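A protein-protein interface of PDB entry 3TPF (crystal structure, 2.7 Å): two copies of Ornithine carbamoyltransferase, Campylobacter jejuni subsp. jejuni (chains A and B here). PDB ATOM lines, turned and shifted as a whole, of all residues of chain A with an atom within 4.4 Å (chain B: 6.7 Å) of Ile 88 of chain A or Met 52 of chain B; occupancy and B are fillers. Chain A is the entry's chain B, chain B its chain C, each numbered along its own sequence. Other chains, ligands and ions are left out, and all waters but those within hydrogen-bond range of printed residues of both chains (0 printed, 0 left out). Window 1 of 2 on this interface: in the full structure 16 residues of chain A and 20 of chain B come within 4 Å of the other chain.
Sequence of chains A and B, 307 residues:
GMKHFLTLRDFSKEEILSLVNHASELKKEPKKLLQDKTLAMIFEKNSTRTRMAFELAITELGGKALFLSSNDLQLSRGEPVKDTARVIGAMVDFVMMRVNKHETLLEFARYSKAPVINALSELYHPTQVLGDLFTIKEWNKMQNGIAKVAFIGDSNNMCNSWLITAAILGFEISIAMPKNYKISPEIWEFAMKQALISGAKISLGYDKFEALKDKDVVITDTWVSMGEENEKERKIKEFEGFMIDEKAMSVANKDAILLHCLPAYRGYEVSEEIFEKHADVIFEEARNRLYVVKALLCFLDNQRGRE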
ATOM      1  N   ALA A  40      11.000 -23.863 -16.336  1.00  0.00           N
ATOM      2  CA  ALA A  40      10.088 -22.965 -15.622  1.00  0.00           C
ATOM      3  C   ALA A  40       9.084 -23.862 -14.998  1.00  0.00           C
ATOM      4  O   ALA A  40       8.568 -24.698 -15.674  1.00  0.00           O
ATOM      5  CB  ALA A  40       9.402 -22.092 -16.619  1.00  0.00           C
ATOM      6  N   ILE A  42       5.478 -23.845 -13.390  1.00  0.00           N
ATOM      7  CA  ILE A  42       4.294 -22.969 -13.011  1.00  0.00           C
ATOM      8  C   ILE A  42       3.251 -23.740 -12.263  1.00  0.00           C
ATOM      9  O   ILE A  42       2.670 -24.665 -12.817  1.00  0.00           O
ATOM     10  CB  ILE A  42       3.566 -22.390 -14.244  1.00  0.00           C
ATOM     11  CG1 ILE A  42       4.514 -21.513 -15.058  1.00  0.00           C
ATOM     12  CG2 ILE A  42       2.348 -21.603 -13.800  1.00  0.00           C
ATOM     13  CD1 ILE A  42       4.000 -21.202 -16.434  1.00  0.00           C
ATOM     14  N   LEU A  68       7.845 -20.735 -10.238  1.00  0.00           N
ATOM     15  CA  LEU A  68       6.839 -19.636 -10.163  1.00  0.00           C
ATOM     16  C   LEU A  68       5.581 -20.134  -9.481  1.00  0.00           C
ATOM     17  O   LEU A  68       4.900 -20.990  -9.966  1.00  0.00           O
ATOM     18  CB  LEU A  68       6.522 -19.092 -11.526  1.00  0.00           C
ATOM     19  CG  LEU A  68       7.802 -19.096 -12.354  1.00  0.00           C
ATOM     20  CD1 LEU A  68       7.552 -18.432 -13.689  1.00  0.00           C
ATOM     21  CD2 LEU A  68       8.960 -18.464 -11.621  1.00  0.00           C
ATOM     22  N   LEU A  73       2.432 -16.161  -9.679  1.00  0.00           N
ATOM     23  CA  LEU A  73       1.853 -16.209 -11.025  1.00  0.00           C
ATOM     24  C   LEU A  73       0.376 -16.528 -10.974  1.00  0.00           C
ATOM     25  O   LEU A  73      -0.020 -17.675 -10.713  1.00  0.00           O
ATOM     26  CB  LEU A  73       2.578 -17.219 -11.940  1.00  0.00           C
ATOM     27  CG  LEU A  73       2.361 -16.981 -13.447  1.00  0.00           C
ATOM     28  CD1 LEU A  73       2.983 -15.663 -13.932  1.00  0.00           C
ATOM     29  CD2 LEU A  73       2.939 -18.161 -14.200  1.00  0.00           C
ATOM     30  N   THR A  84       1.342 -14.763 -21.470  1.00  0.00           N
ATOM     31  CA  THR A  84       2.310 -15.345 -20.564  1.00  0.00           C
ATOM     32  C   THR A  84       3.156 -16.329 -21.347  1.00  0.00           C
ATOM     33  O   THR A  84       4.380 -16.302 -21.278  1.00  0.00           O
ATOM     34  CB  THR A  84       1.635 -16.028 -19.393  1.00  0.00           C
ATOM     35  OG1 THR A  84       0.742 -15.082 -18.793  1.00  0.00           O
ATOM     36  CG2 THR A  84       2.661 -16.519 -18.366  1.00  0.00           C
ATOM     37  N   ALA A  85       2.486 -17.173 -22.107  1.00  0.00           N
ATOM     38  CA  ALA A  85       3.162 -18.188 -22.867  1.00  0.00           C
ATOM     39  C   ALA A  85       4.190 -17.588 -23.755  1.00  0.00           C
ATOM     40  O   ALA A  85       5.304 -18.115 -23.900  1.00  0.00           O
ATOM     41  CB  ALA A  85       2.192 -18.955 -23.679  1.00  0.00           C
ATOM     42  N   ARG A  86       3.862 -16.454 -24.354  1.00  0.00           N
ATOM     43  CA  ARG A  86       4.782 -15.870 -25.377  1.00  0.00           C
ATOM     44  C   ARG A  86       5.965 -15.151 -24.762  1.00  0.00           C
ATOM     45  O   ARG A  86       6.927 -14.876 -25.451  1.00  0.00           O
ATOM     46  CB  ARG A  86       4.075 -14.942 -26.301  1.00  0.00           C
ATOM     47  CG  ARG A  86       3.311 -15.665 -27.377  1.00  0.00           C
ATOM     48  CD  ARG A  86       2.576 -14.694 -28.281  1.00  0.00           C
ATOM     49  NE  ARG A  86       1.386 -14.154 -27.657  1.00  0.00           N
ATOM     50  CZ  ARG A  86       0.508 -13.399 -28.302  1.00  0.00           C
ATOM     51  NH1 ARG A  86       0.684 -13.132 -29.594  1.00  0.00           N
ATOM     52  NH2 ARG A  86      -0.559 -12.903 -27.671  1.00  0.00           N
ATOM     53  N   VAL A  87       5.889 -14.889 -23.461  1.00  0.00           N
ATOM     54  CA  VAL A  87       7.081 -14.457 -22.713  1.00  0.00           C
ATOM     55  C   VAL A  87       7.844 -15.643 -22.116  1.00  0.00           C
ATOM     56  O   VAL A  87       8.987 -15.881 -22.463  1.00  0.00           O
ATOM     57  CB  VAL A  87       6.790 -13.479 -21.532  1.00  0.00           C
ATOM     58  CG1 VAL A  87       8.110 -13.143 -20.847  1.00  0.00           C
ATOM     59  CG2 VAL A  87       6.100 -12.200 -21.953  1.00  0.00           C
ATOM     60  N   ILE A  88       7.236 -16.347 -21.170  1.00  0.00           N
ATOM     61  CA  ILE A  88       7.939 -17.377 -20.389  1.00  0.00           C
ATOM     62  C   ILE A  88       8.441 -18.455 -21.339  1.00  0.00           C
ATOM     63  O   ILE A  88       9.617 -18.878 -21.296  1.00  0.00           O
ATOM     64  CB  ILE A  88       7.051 -18.049 -19.347  1.00  0.00           C
ATOM     65  CG1 ILE A  88       6.735 -17.084 -18.230  1.00  0.00           C
ATOM     66  CG2 ILE A  88       7.750 -19.203 -18.675  1.00  0.00           C
ATOM     67  CD1 ILE A  88       5.594 -17.466 -17.294  1.00  0.00           C
ATOM     68  N   GLY A  89       7.564 -18.889 -22.244  1.00  0.00           N
ATOM     69  CA  GLY A  89       7.935 -19.984 -23.174  1.00  0.00           C
ATOM     70  C   GLY A  89       9.062 -19.648 -24.125  1.00  0.00           C
ATOM     71  O   GLY A  89       9.494 -20.504 -24.933  1.00  0.00           O
ATOM     72  N   ALA A  90       9.471 -18.391 -24.108  1.00  0.00           N
ATOM     73  CA  ALA A  90      10.471 -17.932 -25.050  1.00  0.00           C
ATOM     74  C   ALA A  90      11.778 -17.849 -24.377  1.00  0.00           C
ATOM     75  O   ALA A  90      12.822 -17.776 -25.005  1.00  0.00           O
ATOM     76  CB  ALA A  90      10.087 -16.603 -25.627  1.00  0.00           C
ATOM     77  N   MET A  91      11.734 -17.840 -23.062  1.00  0.00           N
ATOM     78  CA  MET A  91      12.984 -17.604 -22.310  1.00  0.00           C
ATOM     79  C   MET A  91      13.578 -18.828 -21.698  1.00  0.00           C
ATOM     80  O   MET A  91      14.762 -18.811 -21.341  1.00  0.00           O
ATOM     81  CB  MET A  91      12.690 -16.638 -21.213  1.00  0.00           C
ATOM     82  CG  MET A  91      12.198 -15.377 -21.888  1.00  0.00           C
ATOM     83  SD  MET A  91      11.839 -13.950 -20.575  1.00  0.00           S
ATOM     84  CE  MET A  91      13.725 -13.409 -20.269  1.00  0.00           C
ATOM     85  N   VAL A  92      12.773 -19.880 -21.546  1.00  0.00           N
ATOM     86  CA  VAL A  92      13.255 -21.095 -20.899  1.00  0.00           C
ATOM     87  C   VAL A  92      13.262 -22.222 -21.888  1.00  0.00           C
ATOM     88  O   VAL A  92      12.639 -22.138 -22.918  1.00  0.00           O
ATOM     89  CB  VAL A  92      12.425 -21.497 -19.689  1.00  0.00           C
ATOM     90  CG1 VAL A  92      12.473 -20.388 -18.656  1.00  0.00           C
ATOM     91  CG2 VAL A  92      11.043 -21.945 -20.113  1.00  0.00           C
ATOM     92  N   VAL A  95       8.793 -25.961 -19.978  1.00  0.00           N
ATOM     93  CA  VAL A  95       7.872 -25.366 -19.032  1.00  0.00           C
ATOM     94  C   VAL A  95       7.018 -26.437 -18.422  1.00  0.00           C
ATOM     95  O   VAL A  95       6.293 -27.070 -19.184  1.00  0.00           O
ATOM     96  CB  VAL A  95       6.926 -24.372 -19.694  1.00  0.00           C
ATOM     97  CG1 VAL A  95       5.768 -24.026 -18.729  1.00  0.00           C
ATOM     98  CG2 VAL A  95       7.689 -23.156 -20.170  1.00  0.00           C
ATOM     99  N   MET B  41      17.009 -11.055  -4.701  1.00  0.00           N
ATOM    100  CA  MET B  41      15.938 -10.335  -5.377  1.00  0.00           C
ATOM    101  C   MET B  41      14.846 -10.102  -4.417  1.00  0.00           C
ATOM    102  O   MET B  41      14.215 -11.044  -3.933  1.00  0.00           O
ATOM    103  CB  MET B  41      15.374 -11.124  -6.535  1.00  0.00           C
ATOM    104  CG  MET B  41      16.425 -11.484  -7.577  1.00  0.00           C
ATOM    105  SD  MET B  41      15.626 -12.638  -9.004  1.00  0.00           S
ATOM    106  CE  MET B  41      14.989 -14.102  -7.844  1.00  0.00           C
ATOM    107  N   PHE B  43      11.267  -8.656  -3.616  1.00  0.00           N
ATOM    108  CA  PHE B  43       9.993  -8.135  -4.202  1.00  0.00           C
ATOM    109  C   PHE B  43       9.016  -7.687  -3.131  1.00  0.00           C
ATOM    110  O   PHE B  43       8.772  -8.383  -2.159  1.00  0.00           O
ATOM    111  CB  PHE B  43       9.299  -9.161  -5.069  1.00  0.00           C
ATOM    112  CG  PHE B  43      10.046  -9.482  -6.315  1.00  0.00           C
ATOM    113  CD1 PHE B  43      11.085 -10.405  -6.291  1.00  0.00           C
ATOM    114  CD2 PHE B  43       9.733  -8.858  -7.502  1.00  0.00           C
ATOM    115  CE1 PHE B  43      11.792 -10.681  -7.432  1.00  0.00           C
ATOM    116  CE2 PHE B  43      10.448  -9.105  -8.652  1.00  0.00           C
ATOM    117  CZ  PHE B  43      11.464 -10.025  -8.614  1.00  0.00           C
ATOM    118  N   SER B  47       6.293  -9.615  -9.579  1.00  0.00           N
ATOM    119  CA  SER B  47       6.301  -9.441 -11.022  1.00  0.00           C
ATOM    120  C   SER B  47       7.057 -10.609 -11.555  1.00  0.00           C
ATOM    121  O   SER B  47       8.276 -10.629 -11.487  1.00  0.00           O
ATOM    122  CB  SER B  47       7.013  -8.149 -11.465  1.00  0.00           C
ATOM    123  OG  SER B  47       7.321  -8.134 -12.862  1.00  0.00           O
ATOM    124  N   THR B  48       6.325 -11.559 -12.110  1.00  0.00           N
ATOM    125  CA  THR B  48       6.917 -12.727 -12.768  1.00  0.00           C
ATOM    126  C   THR B  48       7.831 -12.322 -13.969  1.00  0.00           C
ATOM    127  O   THR B  48       9.001 -12.724 -14.055  1.00  0.00           O
ATOM    128  CB  THR B  48       5.821 -13.752 -13.210  1.00  0.00           C
ATOM    129  OG1 THR B  48       5.083 -14.207 -12.072  1.00  0.00           O
ATOM    130  CG2 THR B  48       6.429 -14.975 -13.877  1.00  0.00           C
ATOM    131  N   ARG B  49       7.325 -11.498 -14.867  1.00  0.00           N
ATOM    132  CA  ARG B  49       8.165 -11.031 -15.975  1.00  0.00           C
ATOM    133  C   ARG B  49       9.592 -10.543 -15.552  1.00  0.00           C
ATOM    134  O   ARG B  49      10.600 -10.795 -16.232  1.00  0.00           O
ATOM    135  CB  ARG B  49       7.454  -9.896 -16.681  1.00  0.00           C
ATOM    136  CG  ARG B  49       7.793  -9.747 -18.179  1.00  0.00           C
ATOM    137  CD  ARG B  49       6.729  -8.952 -18.960  1.00  0.00           C
ATOM    138  NE  ARG B  49       5.375  -9.536 -18.859  1.00  0.00           N
ATOM    139  CZ  ARG B  49       4.465  -9.245 -17.921  1.00  0.00           C
ATOM    140  NH1 ARG B  49       3.284  -9.848 -17.931  1.00  0.00           N
ATOM    141  NH2 ARG B  49       4.718  -8.353 -16.960  1.00  0.00           N
ATOM    142  N   THR B  50       9.648  -9.822 -14.435  1.00  0.00           N
ATOM    143  CA  THR B  50      10.870  -9.150 -13.974  1.00  0.00           C
ATOM    144  C   THR B  50      11.813 -10.188 -13.422  1.00  0.00           C
ATOM    145  O   THR B  50      13.029 -10.227 -13.648  1.00  0.00           O
ATOM    146  CB  THR B  50      10.560  -8.113 -12.831  1.00  0.00           C
ATOM    147  OG1 THR B  50      10.033  -6.879 -13.352  1.00  0.00           O
ATOM    148  CG2 THR B  50      11.803  -7.747 -12.142  1.00  0.00           C
ATOM    149  N   ARG B  51      11.219 -10.975 -12.581  1.00  0.00           N
ATOM    150  CA  ARG B  51      11.930 -12.000 -11.920  1.00  0.00           C
ATOM    151  C   ARG B  51      12.653 -12.887 -12.909  1.00  0.00           C
ATOM    152  O   ARG B  51      13.773 -13.289 -12.704  1.00  0.00           O
ATOM    153  CB  ARG B  51      10.937 -12.863 -11.160  1.00  0.00           C
ATOM    154  CG  ARG B  51      11.587 -13.809 -10.187  1.00  0.00           C
ATOM    155  CD  ARG B  51      10.707 -14.999  -9.932  1.00  0.00           C
ATOM    156  NE  ARG B  51      11.556 -16.132  -9.707  1.00  0.00           N
ATOM    157  CZ  ARG B  51      11.143 -17.234  -9.138  1.00  0.00           C
ATOM    158  NH1 ARG B  51       9.879 -17.314  -8.735  1.00  0.00           N
ATOM    159  NH2 ARG B  51      12.005 -18.267  -8.972  1.00  0.00           N
ATOM    160  N   MET B  52      11.976 -13.232 -13.972  1.00  0.00           N
ATOM    161  CA  MET B  52      12.551 -14.095 -14.997  1.00  0.00           C
ATOM    162  C   MET B  52      13.811 -13.463 -15.511  1.00  0.00           C
ATOM    163  O   MET B  52      14.881 -14.116 -15.607  1.00  0.00           O
ATOM    164  CB  MET B  52      11.504 -14.150 -16.110  1.00  0.00           C
ATOM    165  CG  MET B  52      11.604 -15.360 -17.017  1.00  0.00           C
ATOM    166  SD  MET B  52      10.274 -16.686 -16.421  1.00  0.00           S
ATOM    167  CE  MET B  52       8.902 -15.276 -16.778  1.00  0.00           C
ATOM    168  N   ALA B  53      13.678 -12.184 -15.872  1.00  0.00           N
ATOM    169  CA  ALA B  53      14.774 -11.414 -16.452  1.00  0.00           C
ATOM    170  C   ALA B  53      16.012 -11.428 -15.566  1.00  0.00           C
ATOM    171  O   ALA B  53      17.140 -11.748 -15.981  1.00  0.00           O
ATOM    172  CB  ALA B  53      14.329 -10.006 -16.680  1.00  0.00           C
ATOM    173  N   PHE B  54      15.785 -11.178 -14.301  1.00  0.00           N
ATOM    174  CA  PHE B  54      16.903 -11.149 -13.390  1.00  0.00           C
ATOM    175  C   PHE B  54      17.435 -12.525 -13.034  1.00  0.00           C
ATOM    176  O   PHE B  54      18.641 -12.739 -13.059  1.00  0.00           O
ATOM    177  CB  PHE B  54      16.540 -10.395 -12.132  1.00  0.00           C
ATOM    178  CG  PHE B  54      16.658  -8.935 -12.281  1.00  0.00           C
ATOM    179  CD1 PHE B  54      17.808  -8.326 -11.996  1.00  0.00           C
ATOM    180  CD2 PHE B  54      15.603  -8.202 -12.727  1.00  0.00           C
ATOM    181  CE1 PHE B  54      17.931  -6.966 -12.129  1.00  0.00           C
ATOM    182  CE2 PHE B  54      15.684  -6.843 -12.829  1.00  0.00           C
ATOM    183  CZ  PHE B  54      16.860  -6.214 -12.529  1.00  0.00           C
ATOM    184  N   GLU B  55      16.544 -13.428 -12.703  1.00  0.00           N
ATOM    185  CA  GLU B  55      16.976 -14.724 -12.312  1.00  0.00           C
ATOM    186  C   GLU B  55      17.816 -15.330 -13.450  1.00  0.00           C
ATOM    187  O   GLU B  55      18.865 -15.964 -13.220  1.00  0.00           O
ATOM    188  CB  GLU B  55      15.796 -15.609 -11.930  1.00  0.00           C
ATOM    189  CG  GLU B  55      16.295 -16.888 -11.274  1.00  0.00           C
ATOM    190  CD  GLU B  55      15.300 -17.574 -10.340  1.00  0.00           C
ATOM    191  OE1 GLU B  55      14.189 -16.987 -10.108  1.00  0.00           O
ATOM    192  OE2 GLU B  55      15.642 -18.731  -9.894  1.00  0.00           O
ATOM    193  N   LEU B  56      17.326 -15.171 -14.697  1.00  0.00           N
ATOM    194  CA  LEU B  56      18.024 -15.783 -15.817  1.00  0.00           C
ATOM    195  C   LEU B  56      19.285 -14.995 -16.129  1.00  0.00           C
ATOM    196  O   LEU B  56      20.316 -15.575 -16.530  1.00  0.00           O
ATOM    197  CB  LEU B  56      17.129 -15.920 -17.041  1.00  0.00           C
ATOM    198  CG  LEU B  56      16.004 -16.984 -17.076  1.00  0.00           C
ATOM    199  CD1 LEU B  56      15.156 -16.828 -18.333  1.00  0.00           C
ATOM    200  CD2 LEU B  56      16.451 -18.399 -16.955  1.00  0.00           C
ATOM    201  N   ALA B  57      19.240 -13.673 -15.904  1.00  0.00           N
ATOM    202  CA  ALA B  57      20.423 -12.860 -16.187  1.00  0.00           C
ATOM    203  C   ALA B  57      21.628 -13.405 -15.367  1.00  0.00           C
ATOM    204  O   ALA B  57      22.643 -13.870 -15.923  1.00  0.00           O
ATOM    205  CB  ALA B  57      20.176 -11.413 -15.949  1.00  0.00           C
ATOM    206  N   LEU B 290      16.325  -9.352 -20.559  1.00  0.00           N
ATOM    207  CA  LEU B 290      17.345 -10.281 -20.097  1.00  0.00           C
ATOM    208  C   LEU B 290      18.739  -9.773 -20.421  1.00  0.00           C
ATOM    209  O   LEU B 290      19.592  -9.711 -19.563  1.00  0.00           O
ATOM    210  CB  LEU B 290      17.166 -11.644 -20.742  1.00  0.00           C
ATOM    211  CG  LEU B 290      18.289 -12.625 -20.352  1.00  0.00           C
ATOM    212  CD1 LEU B 290      18.435 -12.800 -18.830  1.00  0.00           C
ATOM    213  CD2 LEU B 290      18.044 -13.960 -21.006  1.00  0.00           C
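Ala 40 of chain A touches none of the printed residues of chain B. Of chain B, only Met 52 comes within 4 Å of Ile 88 of chain A. Printed residues of chain B within 4 Å of Met 91 of chain A: Met 52 (3.8 Å), Leu 56 (3.6 Å) and Leu 290 (3.9 Å). Of the printed residues of chain A, Arg 51 of chain B touches Leu 68 (3.2 Å). Printed residues of chain A within 4 Å of Leu 56 of chain B: Met 91. The nearest residue of chain B that does not touch Ile 88 of chain A is Thr 48 of chain B (4.3 Å).
Of the 14 printed residues of chain A, 4 touch a printed residue of chain B. Hydrophobic or aromatic side chains of chain A that line the printed part of chain B: Leu 68, Leu 73, Ile 88 and Met 91. Of the 14 printed residues of chain B, 5 touch a printed residue of chain A. Along chain B the printed residues that touch a printed residue of chain A span positions 48 to 290. Among the printed residues, no Asp or Glu carboxylate lies within 4 Å of a Lys or Arg side-chain nitrogen of the other chain.
OE1 of Glu 55 of chain B lies within salt-bridge range of NH2 of Arg 51 of chain B, 2.8 Å away.
No position is printed for both chains. Of the 7 pairs that touch across the chains among the printed residues, none has its exchanged pair printed and touching as well.
Leu 68 of chain A touches Thr 48 of chain B (CD1 to CG2, 3.6 Å). Arg 51 of chain B touches Leu 68 of chain A. CD1 of Leu 73 of chain A touches OG1 of Thr 48 of chain B, at 3.2 Å. CE of Met 52 of chain B touches CG1 of Ile 88 of chain A (3.2 Å). Met 52 of chain B touches Met 91 of chain A. CD1 of Leu 56 of chain B touches O of Met 91 of chain A, at 3.6 Å. Met 91 of chain A touches Leu 290 of chain B.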
